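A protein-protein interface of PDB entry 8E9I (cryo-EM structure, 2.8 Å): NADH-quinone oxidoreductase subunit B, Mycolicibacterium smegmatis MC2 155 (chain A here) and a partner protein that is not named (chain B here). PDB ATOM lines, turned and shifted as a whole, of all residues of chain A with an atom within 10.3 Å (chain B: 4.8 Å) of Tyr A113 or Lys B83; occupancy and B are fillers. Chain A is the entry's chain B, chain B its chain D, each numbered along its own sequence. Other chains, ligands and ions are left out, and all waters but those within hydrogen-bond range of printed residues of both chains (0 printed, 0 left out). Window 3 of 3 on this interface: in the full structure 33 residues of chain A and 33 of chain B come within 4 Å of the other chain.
The backbone carbonyl oxygen of Phe A110 sits at hydrogen-bond distance from the side-chain amide nitrogen of Gln A117 (2.8 Å).
The backbone NH (N) of Lys A79 lies close to the side-chain hydroxyl (OG) of Ser A77 (3.3 Å).
The side-chain hydroxyl (OG) of Ser A77 sits at hydrogen-bond distance from the backbone NH (N) of Met A80, 3.2 Å away.
NE2 of Gln A78 sits at hydrogen-bond distance from O of Tyr A113, at 3.0 Å.
The backbone NH of Gln A78 is in hydrogen-bond range of the backbone carbonyl oxygen of Ala A114, 2.8 Å away.
The side-chain amide nitrogen (NE2) of Gln A117 sits close to the backbone NH (N) of Asn A112, at 3.3 Å.
Among the printed residues, pairs that only touch across the chains: Ser A77 with His B78, Met A109 with Asn B84, Phe A110 with Ile B81, Phe A110 with Asn B84, Asn A111 with Asn B84, Asn A112 with Asn B84, Tyr A113 with His B78, Tyr A113 with Gly B80, Tyr A113 with Lys B83, Ala A114 with His B78 and Ala A114 with Gly B80.
Of chain B, only His B78 (3.0 Å), Gly B80 (3.9 Å) and Lys B83 (3.8 Å) come within 4 Å of Tyr A113.
Of chain A, only Tyr A113 (3.8 Å) comes within 4 Å of Lys B83.
Of the printed residues of chain A, Gly B80 touches Tyr A113 and Ala A114.
Glu B86 touches none of the printed residues of chain A.
Of the printed residues of chain B, Asn A112 touches Asn B84 (3.4 Å).
Of the printed residues of chain B, Ser A77 touches His B78.
Tyr B87 touches none of the printed residues of chain A.
Gln A78 touches none of the printed residues of chain B.
The nearest printed residue of chain B that does not touch Tyr A113 is Ile B81 (6.0 Å).
The nearest residue of chain A that does not touch Lys B83 is Asn A112 (6.6 Å).
The nearest printed residue of chain B that does not touch Met A109 is Ile B81 (6.1 Å).
Of the 9 printed residues of chain B, 5 touch a printed residue of chain A.
Of the 19 printed residues of chain A, 7 touch a printed residue of chain B.
Printed residues of chain A that touch a printed residue of chain B: Ser A77, Met A109, Phe A110, Asn A111, Asn A112, Tyr A113 and Ala A114.
Among the printed residues, 11 pairs touch across the chains.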
ATOM      1  N   VAL A  76       7.631 -15.541 -19.164  1.00  0.00           N
ATOM      2  CA  VAL A  76       8.698 -14.607 -18.836  1.00  0.00           C
ATOM      3  C   VAL A  76      10.021 -15.344 -18.963  1.00  0.00           C
ATOM      4  O   VAL A  76      10.425 -16.071 -18.056  1.00  0.00           O
ATOM      5  CB  VAL A  76       8.523 -14.032 -17.428  1.00  0.00           C
ATOM      6  CG1 VAL A  76       9.682 -13.119 -17.081  1.00  0.00           C
ATOM      7  CG2 VAL A  76       7.216 -13.297 -17.333  1.00  0.00           C
ATOM      8  N   SER A  77      10.700 -15.150 -20.086  1.00  0.00           N
ATOM      9  CA  SER A  77      12.043 -15.679 -20.217  1.00  0.00           C
ATOM     10  C   SER A  77      12.965 -14.990 -19.223  1.00  0.00           C
ATOM     11  O   SER A  77      12.600 -14.016 -18.565  1.00  0.00           O
ATOM     12  CB  SER A  77      12.567 -15.474 -21.634  1.00  0.00           C
ATOM     13  OG  SER A  77      12.986 -14.139 -21.824  1.00  0.00           O
ATOM     14  N   GLN A  78      14.182 -15.518 -19.109  1.00  0.00           N
ATOM     15  CA  GLN A  78      15.172 -14.889 -18.246  1.00  0.00           C
ATOM     16  C   GLN A  78      15.474 -13.478 -18.721  1.00  0.00           C
ATOM     17  O   GLN A  78      15.502 -12.532 -17.930  1.00  0.00           O
ATOM     18  CB  GLN A  78      16.447 -15.729 -18.223  1.00  0.00           C
ATOM     19  CG  GLN A  78      16.238 -17.117 -17.686  1.00  0.00           C
ATOM     20  CD  GLN A  78      16.005 -17.127 -16.203  1.00  0.00           C
ATOM     21  OE1 GLN A  78      15.992 -16.085 -15.561  1.00  0.00           O
ATOM     22  NE2 GLN A  78      15.799 -18.310 -15.648  1.00  0.00           N
ATOM     23  N   LYS A  79      15.680 -13.318 -20.027  1.00  0.00           N
ATOM     24  CA  LYS A  79      16.054 -12.019 -20.566  1.00  0.00           C
ATOM     25  C   LYS A  79      14.917 -11.017 -20.481  1.00  0.00           C
ATOM     26  O   LYS A  79      15.146  -9.819 -20.670  1.00  0.00           O
ATOM     27  CB  LYS A  79      16.508 -12.181 -22.014  1.00  0.00           C
ATOM     28  CG  LYS A  79      17.474 -11.126 -22.465  1.00  0.00           C
ATOM     29  CD  LYS A  79      18.392 -11.638 -23.545  1.00  0.00           C
ATOM     30  CE  LYS A  79      17.669 -11.803 -24.853  1.00  0.00           C
ATOM     31  NZ  LYS A  79      18.585 -12.262 -25.927  1.00  0.00           N
ATOM     32  N   MET A  80      13.701 -11.480 -20.206  1.00  0.00           N
ATOM     33  CA  MET A  80      12.545 -10.603 -20.130  1.00  0.00           C
ATOM     34  C   MET A  80      12.229 -10.188 -18.706  1.00  0.00           C
ATOM     35  O   MET A  80      11.607  -9.142 -18.495  1.00  0.00           O
ATOM     36  CB  MET A  80      11.329 -11.301 -20.740  1.00  0.00           C
ATOM     37  CG  MET A  80      10.092 -10.446 -20.841  1.00  0.00           C
ATOM     38  SD  MET A  80      10.260  -9.202 -22.129  1.00  0.00           S
ATOM     39  CE  MET A  80       9.454  -7.817 -21.349  1.00  0.00           C
ATOM     40  N   ALA A  81      12.641 -10.982 -17.726  1.00  0.00           N
ATOM     41  CA  ALA A  81      12.380 -10.637 -16.335  1.00  0.00           C
ATOM     42  C   ALA A  81      12.868  -9.247 -15.968  1.00  0.00           C
ATOM     43  O   ALA A  81      12.104  -8.506 -15.330  1.00  0.00           O
ATOM     44  CB  ALA A  81      13.019 -11.684 -15.419  1.00  0.00           C
ATOM     45  N   GLY A 107       5.463 -20.949 -14.683  1.00  0.00           N
ATOM     46  CA  GLY A 107       6.331 -21.510 -15.691  1.00  0.00           C
ATOM     47  C   GLY A 107       5.649 -22.477 -16.627  1.00  0.00           C
ATOM     48  O   GLY A 107       6.176 -22.743 -17.711  1.00  0.00           O
ATOM     49  N   GLY A 108       4.492 -23.004 -16.247  1.00  0.00           N
ATOM     50  CA  GLY A 108       3.756 -23.871 -17.142  1.00  0.00           C
ATOM     51  C   GLY A 108       4.577 -25.067 -17.563  1.00  0.00           C
ATOM     52  O   GLY A 108       5.475 -25.525 -16.850  1.00  0.00           O
ATOM     53  N   MET A 109       4.268 -25.577 -18.753  1.00  0.00           N
ATOM     54  CA  MET A 109       4.957 -26.751 -19.271  1.00  0.00           C
ATOM     55  C   MET A 109       6.448 -26.510 -19.441  1.00  0.00           C
ATOM     56  O   MET A 109       7.240 -27.456 -19.387  1.00  0.00           O
ATOM     57  CB  MET A 109       4.328 -27.145 -20.599  1.00  0.00           C
ATOM     58  CG  MET A 109       4.930 -28.352 -21.266  1.00  0.00           C
ATOM     59  SD  MET A 109       4.051 -28.704 -22.792  1.00  0.00           S
ATOM     60  CE  MET A 109       4.579 -27.327 -23.786  1.00  0.00           C
ATOM     61  N   PHE A 110       6.851 -25.260 -19.645  1.00  0.00           N
ATOM     62  CA  PHE A 110       8.235 -24.936 -19.969  1.00  0.00           C
ATOM     63  C   PHE A 110       9.077 -24.811 -18.697  1.00  0.00           C
ATOM     64  O   PHE A 110       9.608 -23.759 -18.357  1.00  0.00           O
ATOM     65  CB  PHE A 110       8.270 -23.664 -20.800  1.00  0.00           C
ATOM     66  CG  PHE A 110       7.461 -23.757 -22.048  1.00  0.00           C
ATOM     67  CD1 PHE A 110       7.754 -24.709 -23.000  1.00  0.00           C
ATOM     68  CD2 PHE A 110       6.393 -22.914 -22.263  1.00  0.00           C
ATOM     69  CE1 PHE A 110       7.008 -24.808 -24.150  1.00  0.00           C
ATOM     70  CE2 PHE A 110       5.644 -23.010 -23.412  1.00  0.00           C
ATOM     71  CZ  PHE A 110       5.950 -23.960 -24.354  1.00  0.00           C
ATOM     72  N   ASN A 111       9.178 -25.935 -17.991  1.00  0.00           N
ATOM     73  CA  ASN A 111      10.042 -26.055 -16.819  1.00  0.00           C
ATOM     74  C   ASN A 111      11.481 -26.205 -17.307  1.00  0.00           C
ATOM     75  O   ASN A 111      12.018 -27.303 -17.458  1.00  0.00           O
ATOM     76  CB  ASN A 111       9.604 -27.233 -15.965  1.00  0.00           C
ATOM     77  CG  ASN A 111      10.252 -27.238 -14.606  1.00  0.00           C
ATOM     78  OD1 ASN A 111      10.987 -26.325 -14.251  1.00  0.00           O
ATOM     79  ND2 ASN A 111       9.969 -28.268 -13.829  1.00  0.00           N
ATOM     80  N   ASN A 112      12.105 -25.062 -17.572  1.00  0.00           N
ATOM     81  CA  ASN A 112      13.381 -25.039 -18.265  1.00  0.00           C
ATOM     82  C   ASN A 112      14.260 -23.935 -17.707  1.00  0.00           C
ATOM     83  O   ASN A 112      13.851 -23.149 -16.853  1.00  0.00           O
ATOM     84  CB  ASN A 112      13.194 -24.836 -19.775  1.00  0.00           C
ATOM     85  N   TYR A 113      15.493 -23.902 -18.208  1.00  0.00           N
ATOM     86  CA  TYR A 113      16.413 -22.823 -17.877  1.00  0.00           C
ATOM     87  C   TYR A 113      15.900 -21.483 -18.380  1.00  0.00           C
ATOM     88  O   TYR A 113      16.005 -20.467 -17.686  1.00  0.00           O
ATOM     89  CB  TYR A 113      17.783 -23.117 -18.485  1.00  0.00           C
ATOM     90  CG  TYR A 113      17.766 -23.092 -19.994  1.00  0.00           C
ATOM     91  CD1 TYR A 113      17.287 -24.170 -20.715  1.00  0.00           C
ATOM     92  CD2 TYR A 113      18.199 -21.981 -20.695  1.00  0.00           C
ATOM     93  CE1 TYR A 113      17.256 -24.152 -22.084  1.00  0.00           C
ATOM     94  CE2 TYR A 113      18.174 -21.955 -22.066  1.00  0.00           C
ATOM     95  CZ  TYR A 113      17.693 -23.041 -22.756  1.00  0.00           C
ATOM     96  OH  TYR A 113      17.663 -23.030 -24.129  1.00  0.00           O
ATOM     97  N   ALA A 114      15.348 -21.459 -19.592  1.00  0.00           N
ATOM     98  CA  ALA A 114      15.053 -20.198 -20.252  1.00  0.00           C
ATOM     99  C   ALA A 114      13.922 -19.431 -19.585  1.00  0.00           C
ATOM    100  O   ALA A 114      13.863 -18.207 -19.720  1.00  0.00           O
ATOM    101  CB  ALA A 114      14.706 -20.451 -21.718  1.00  0.00           C
ATOM    102  N   VAL A 115      13.037 -20.109 -18.866  1.00  0.00           N
ATOM    103  CA  VAL A 115      11.813 -19.508 -18.356  1.00  0.00           C
ATOM    104  C   VAL A 115      11.948 -19.313 -16.855  1.00  0.00           C
ATOM    105  O   VAL A 115      12.483 -20.174 -16.152  1.00  0.00           O
ATOM    106  CB  VAL A 115      10.586 -20.376 -18.684  1.00  0.00           C
ATOM    107  CG1 VAL A 115       9.340 -19.770 -18.091  1.00  0.00           C
ATOM    108  CG2 VAL A 115      10.446 -20.543 -20.184  1.00  0.00           C
ATOM    109  N   VAL A 116      11.445 -18.179 -16.365  1.00  0.00           N
ATOM    110  CA  VAL A 116      11.618 -17.813 -14.961  1.00  0.00           C
ATOM    111  C   VAL A 116      10.834 -18.693 -14.003  1.00  0.00           C
ATOM    112  O   VAL A 116      11.154 -18.722 -12.808  1.00  0.00           O
ATOM    113  CB  VAL A 116      11.216 -16.341 -14.761  1.00  0.00           C
ATOM    114  CG1 VAL A 116      11.193 -15.988 -13.293  1.00  0.00           C
ATOM    115  CG2 VAL A 116      12.177 -15.441 -15.499  1.00  0.00           C
ATOM    116  N   GLN A 117       9.833 -19.421 -14.485  1.00  0.00           N
ATOM    117  CA  GLN A 117       8.997 -20.265 -13.632  1.00  0.00           C
ATOM    118  C   GLN A 117       8.141 -19.424 -12.688  1.00  0.00           C
ATOM    119  O   GLN A 117       8.162 -19.614 -11.473  1.00  0.00           O
ATOM    120  CB  GLN A 117       9.836 -21.274 -12.843  1.00  0.00           C
ATOM    121  CG  GLN A 117      10.795 -22.090 -13.688  1.00  0.00           C
ATOM    122  CD  GLN A 117      10.108 -22.784 -14.843  1.00  0.00           C
ATOM    123  OE1 GLN A 117       9.158 -23.536 -14.651  1.00  0.00           O
ATOM    124  NE2 GLN A 117      10.586 -22.535 -16.051  1.00  0.00           N
ATOM    125  N   GLY A 118       7.385 -18.490 -13.252  1.00  0.00           N
ATOM    126  CA  GLY A 118       6.468 -17.690 -12.470  1.00  0.00           C
ATOM    127  C   GLY A 118       6.955 -16.273 -12.287  1.00  0.00           C
ATOM    128  O   GLY A 118       8.044 -16.049 -11.758  1.00  0.00           O
ATOM    129  N   HIS A 121       8.464 -14.581  -9.160  1.00  0.00           N
ATOM    130  CA  HIS A 121       9.881 -14.439  -8.871  1.00  0.00           C
ATOM    131  C   HIS A 121      10.333 -12.990  -8.956  1.00  0.00           C
ATOM    132  O   HIS A 121      11.291 -12.601  -8.281  1.00  0.00           O
ATOM    133  CB  HIS A 121      10.696 -15.289  -9.841  1.00  0.00           C
ATOM    134  CG  HIS A 121      10.676 -16.748  -9.523  1.00  0.00           C
ATOM    135  ND1 HIS A 121      11.717 -17.386  -8.887  1.00  0.00           N
ATOM    136  CD2 HIS A 121       9.738 -17.694  -9.755  1.00  0.00           C
ATOM    137  CE1 HIS A 121      11.422 -18.665  -8.741  1.00  0.00           C
ATOM    138  NE2 HIS A 121      10.225 -18.878  -9.258  1.00  0.00           N
ATOM    139  N   HIS B  78      12.456 -16.148 -25.466  1.00  0.00           N
ATOM    140  CA  HIS B  78      13.057 -17.468 -25.538  1.00  0.00           C
ATOM    141  C   HIS B  78      12.500 -18.347 -24.432  1.00  0.00           C
ATOM    142  O   HIS B  78      12.419 -17.933 -23.275  1.00  0.00           O
ATOM    143  CB  HIS B  78      14.571 -17.371 -25.417  1.00  0.00           C
ATOM    144  CG  HIS B  78      15.262 -18.686 -25.562  1.00  0.00           C
ATOM    145  ND1 HIS B  78      16.083 -19.205 -24.587  1.00  0.00           N
ATOM    146  CD2 HIS B  78      15.257 -19.587 -26.569  1.00  0.00           C
ATOM    147  CE1 HIS B  78      16.550 -20.372 -24.985  1.00  0.00           C
ATOM    148  NE2 HIS B  78      16.065 -20.627 -26.186  1.00  0.00           N
ATOM    149  N   GLY B  80      13.124 -22.137 -24.410  1.00  0.00           N
ATOM    150  CA  GLY B  80      13.760 -23.423 -24.234  1.00  0.00           C
ATOM    151  C   GLY B  80      12.996 -24.577 -24.828  1.00  0.00           C
ATOM    152  O   GLY B  80      13.253 -25.729 -24.471  1.00  0.00           O
ATOM    153  N   ILE B  81      12.069 -24.306 -25.745  1.00  0.00           N
ATOM    154  CA  ILE B  81      11.244 -25.369 -26.305  1.00  0.00           C
ATOM    155  C   ILE B  81      12.106 -26.378 -27.045  1.00  0.00           C
ATOM    156  O   ILE B  81      11.918 -27.590 -26.912  1.00  0.00           O
ATOM    157  CB  ILE B  81      10.161 -24.775 -27.221  1.00  0.00           C
ATOM    158  CG1 ILE B  81       9.468 -23.601 -26.525  1.00  0.00           C
ATOM    159  CG2 ILE B  81       9.162 -25.842 -27.607  1.00  0.00           C
ATOM    160  CD1 ILE B  81       8.263 -23.059 -27.253  1.00  0.00           C
ATOM    161  N   GLU B  82      13.060 -25.896 -27.843  1.00  0.00           N
ATOM    162  CA  GLU B  82      13.873 -26.806 -28.638  1.00  0.00           C
ATOM    163  C   GLU B  82      14.635 -27.784 -27.760  1.00  0.00           C
ATOM    164  O   GLU B  82      14.888 -28.919 -28.174  1.00  0.00           O
ATOM    165  CB  GLU B  82      14.839 -26.016 -29.515  1.00  0.00           C
ATOM    166  N   LYS B  83      15.009 -27.373 -26.551  1.00  0.00           N
ATOM    167  CA  LYS B  83      15.679 -28.280 -25.631  1.00  0.00           C
ATOM    168  C   LYS B  83      14.680 -29.033 -24.767  1.00  0.00           C
ATOM    169  O   LYS B  83      14.843 -30.231 -24.530  1.00  0.00           O
ATOM    170  CB  LYS B  83      16.660 -27.516 -24.742  1.00  0.00           C
ATOM    171  CG  LYS B  83      17.623 -28.430 -24.018  1.00  0.00           C
ATOM    172  CD  LYS B  83      18.337 -27.731 -22.889  1.00  0.00           C
ATOM    173  CE  LYS B  83      19.233 -28.697 -22.147  1.00  0.00           C
ATOM    174  NZ  LYS B  83      20.368 -29.149 -22.993  1.00  0.00           N
ATOM    175  N   ASN B  84      13.643 -28.348 -24.293  1.00  0.00           N
ATOM    176  CA  ASN B  84      12.663 -29.009 -23.445  1.00  0.00           C
ATOM    177  C   ASN B  84      12.024 -30.191 -24.159  1.00  0.00           C
ATOM    178  O   ASN B  84      11.686 -31.192 -23.523  1.00  0.00           O
ATOM    179  CB  ASN B  84      11.595 -28.011 -23.009  1.00  0.00           C
ATOM    180  CG  ASN B  84      11.117 -28.251 -21.602  1.00  0.00           C
ATOM    181  OD1 ASN B  84      10.911 -29.388 -21.191  1.00  0.00           O
ATOM    182  ND2 ASN B  84      10.916 -27.176 -20.858  1.00  0.00           N
ATOM    183  N   LEU B  85      11.855 -30.095 -25.475  1.00  0.00           N
ATOM    184  CA  LEU B  85      11.337 -31.192 -26.278  1.00  0.00           C
ATOM    185  C   LEU B  85      12.105 -32.475 -26.023  1.00  0.00           C
ATOM    186  O   LEU B  85      11.515 -33.551 -25.919  1.00  0.00           O
ATOM    187  CB  LEU B  85      11.430 -30.849 -27.763  1.00  0.00           C
ATOM    188  CG  LEU B  85      10.367 -29.920 -28.327  1.00  0.00           C
ATOM    189  CD1 LEU B  85      10.828 -29.326 -29.638  1.00  0.00           C
ATOM    190  CD2 LEU B  85       9.085 -30.685 -28.525  1.00  0.00           C
ATOM    191  N   GLU B  86      13.425 -32.367 -25.911  1.00  0.00           N
ATOM    192  CA  GLU B  86      14.269 -33.552 -25.906  1.00  0.00           C
ATOM    193  C   GLU B  86      13.994 -34.462 -24.721  1.00  0.00           C
ATOM    194  O   GLU B  86      14.433 -35.615 -24.735  1.00  0.00           O
ATOM    195  CB  GLU B  86      15.737 -33.136 -25.919  1.00  0.00           C
ATOM    196  CG  GLU B  86      16.094 -32.259 -27.100  1.00  0.00           C
ATOM    197  CD  GLU B  86      17.535 -31.812 -27.080  1.00  0.00           C
ATOM    198  OE1 GLU B  86      18.292 -32.292 -26.214  1.00  0.00           O
ATOM    199  OE2 GLU B  86      17.910 -30.978 -27.929  1.00  0.00           O
ATOM    200  N   TYR B  87      13.291 -33.982 -23.703  1.00  0.00           N
ATOM    201  CA  TYR B  87      12.980 -34.782 -22.530  1.00  0.00           C
ATOM    202  C   TYR B  87      11.541 -35.269 -22.525  1.00  0.00           C
ATOM    203  O   TYR B  87      11.007 -35.589 -21.461  1.00  0.00           O
ATOM    204  CB  TYR B  87      13.275 -33.980 -21.267  1.00  0.00           C
ATOM    205  CG  TYR B  87      14.720 -33.564 -21.186  1.00  0.00           C
ATOM    206  CD1 TYR B  87      15.674 -34.402 -20.637  1.00  0.00           C
ATOM    207  CD2 TYR B  87      15.133 -32.341 -21.679  1.00  0.00           C
ATOM    208  CE1 TYR B  87      16.993 -34.031 -20.577  1.00  0.00           C
ATOM    209  CE2 TYR B  87      16.448 -31.963 -21.620  1.00  0.00           C
ATOM    210  CZ  TYR B  87      17.374 -32.811 -21.068  1.00  0.00           C
ATOM    211  OH  TYR B  87      18.689 -32.430 -21.008  1.00  0.00           O
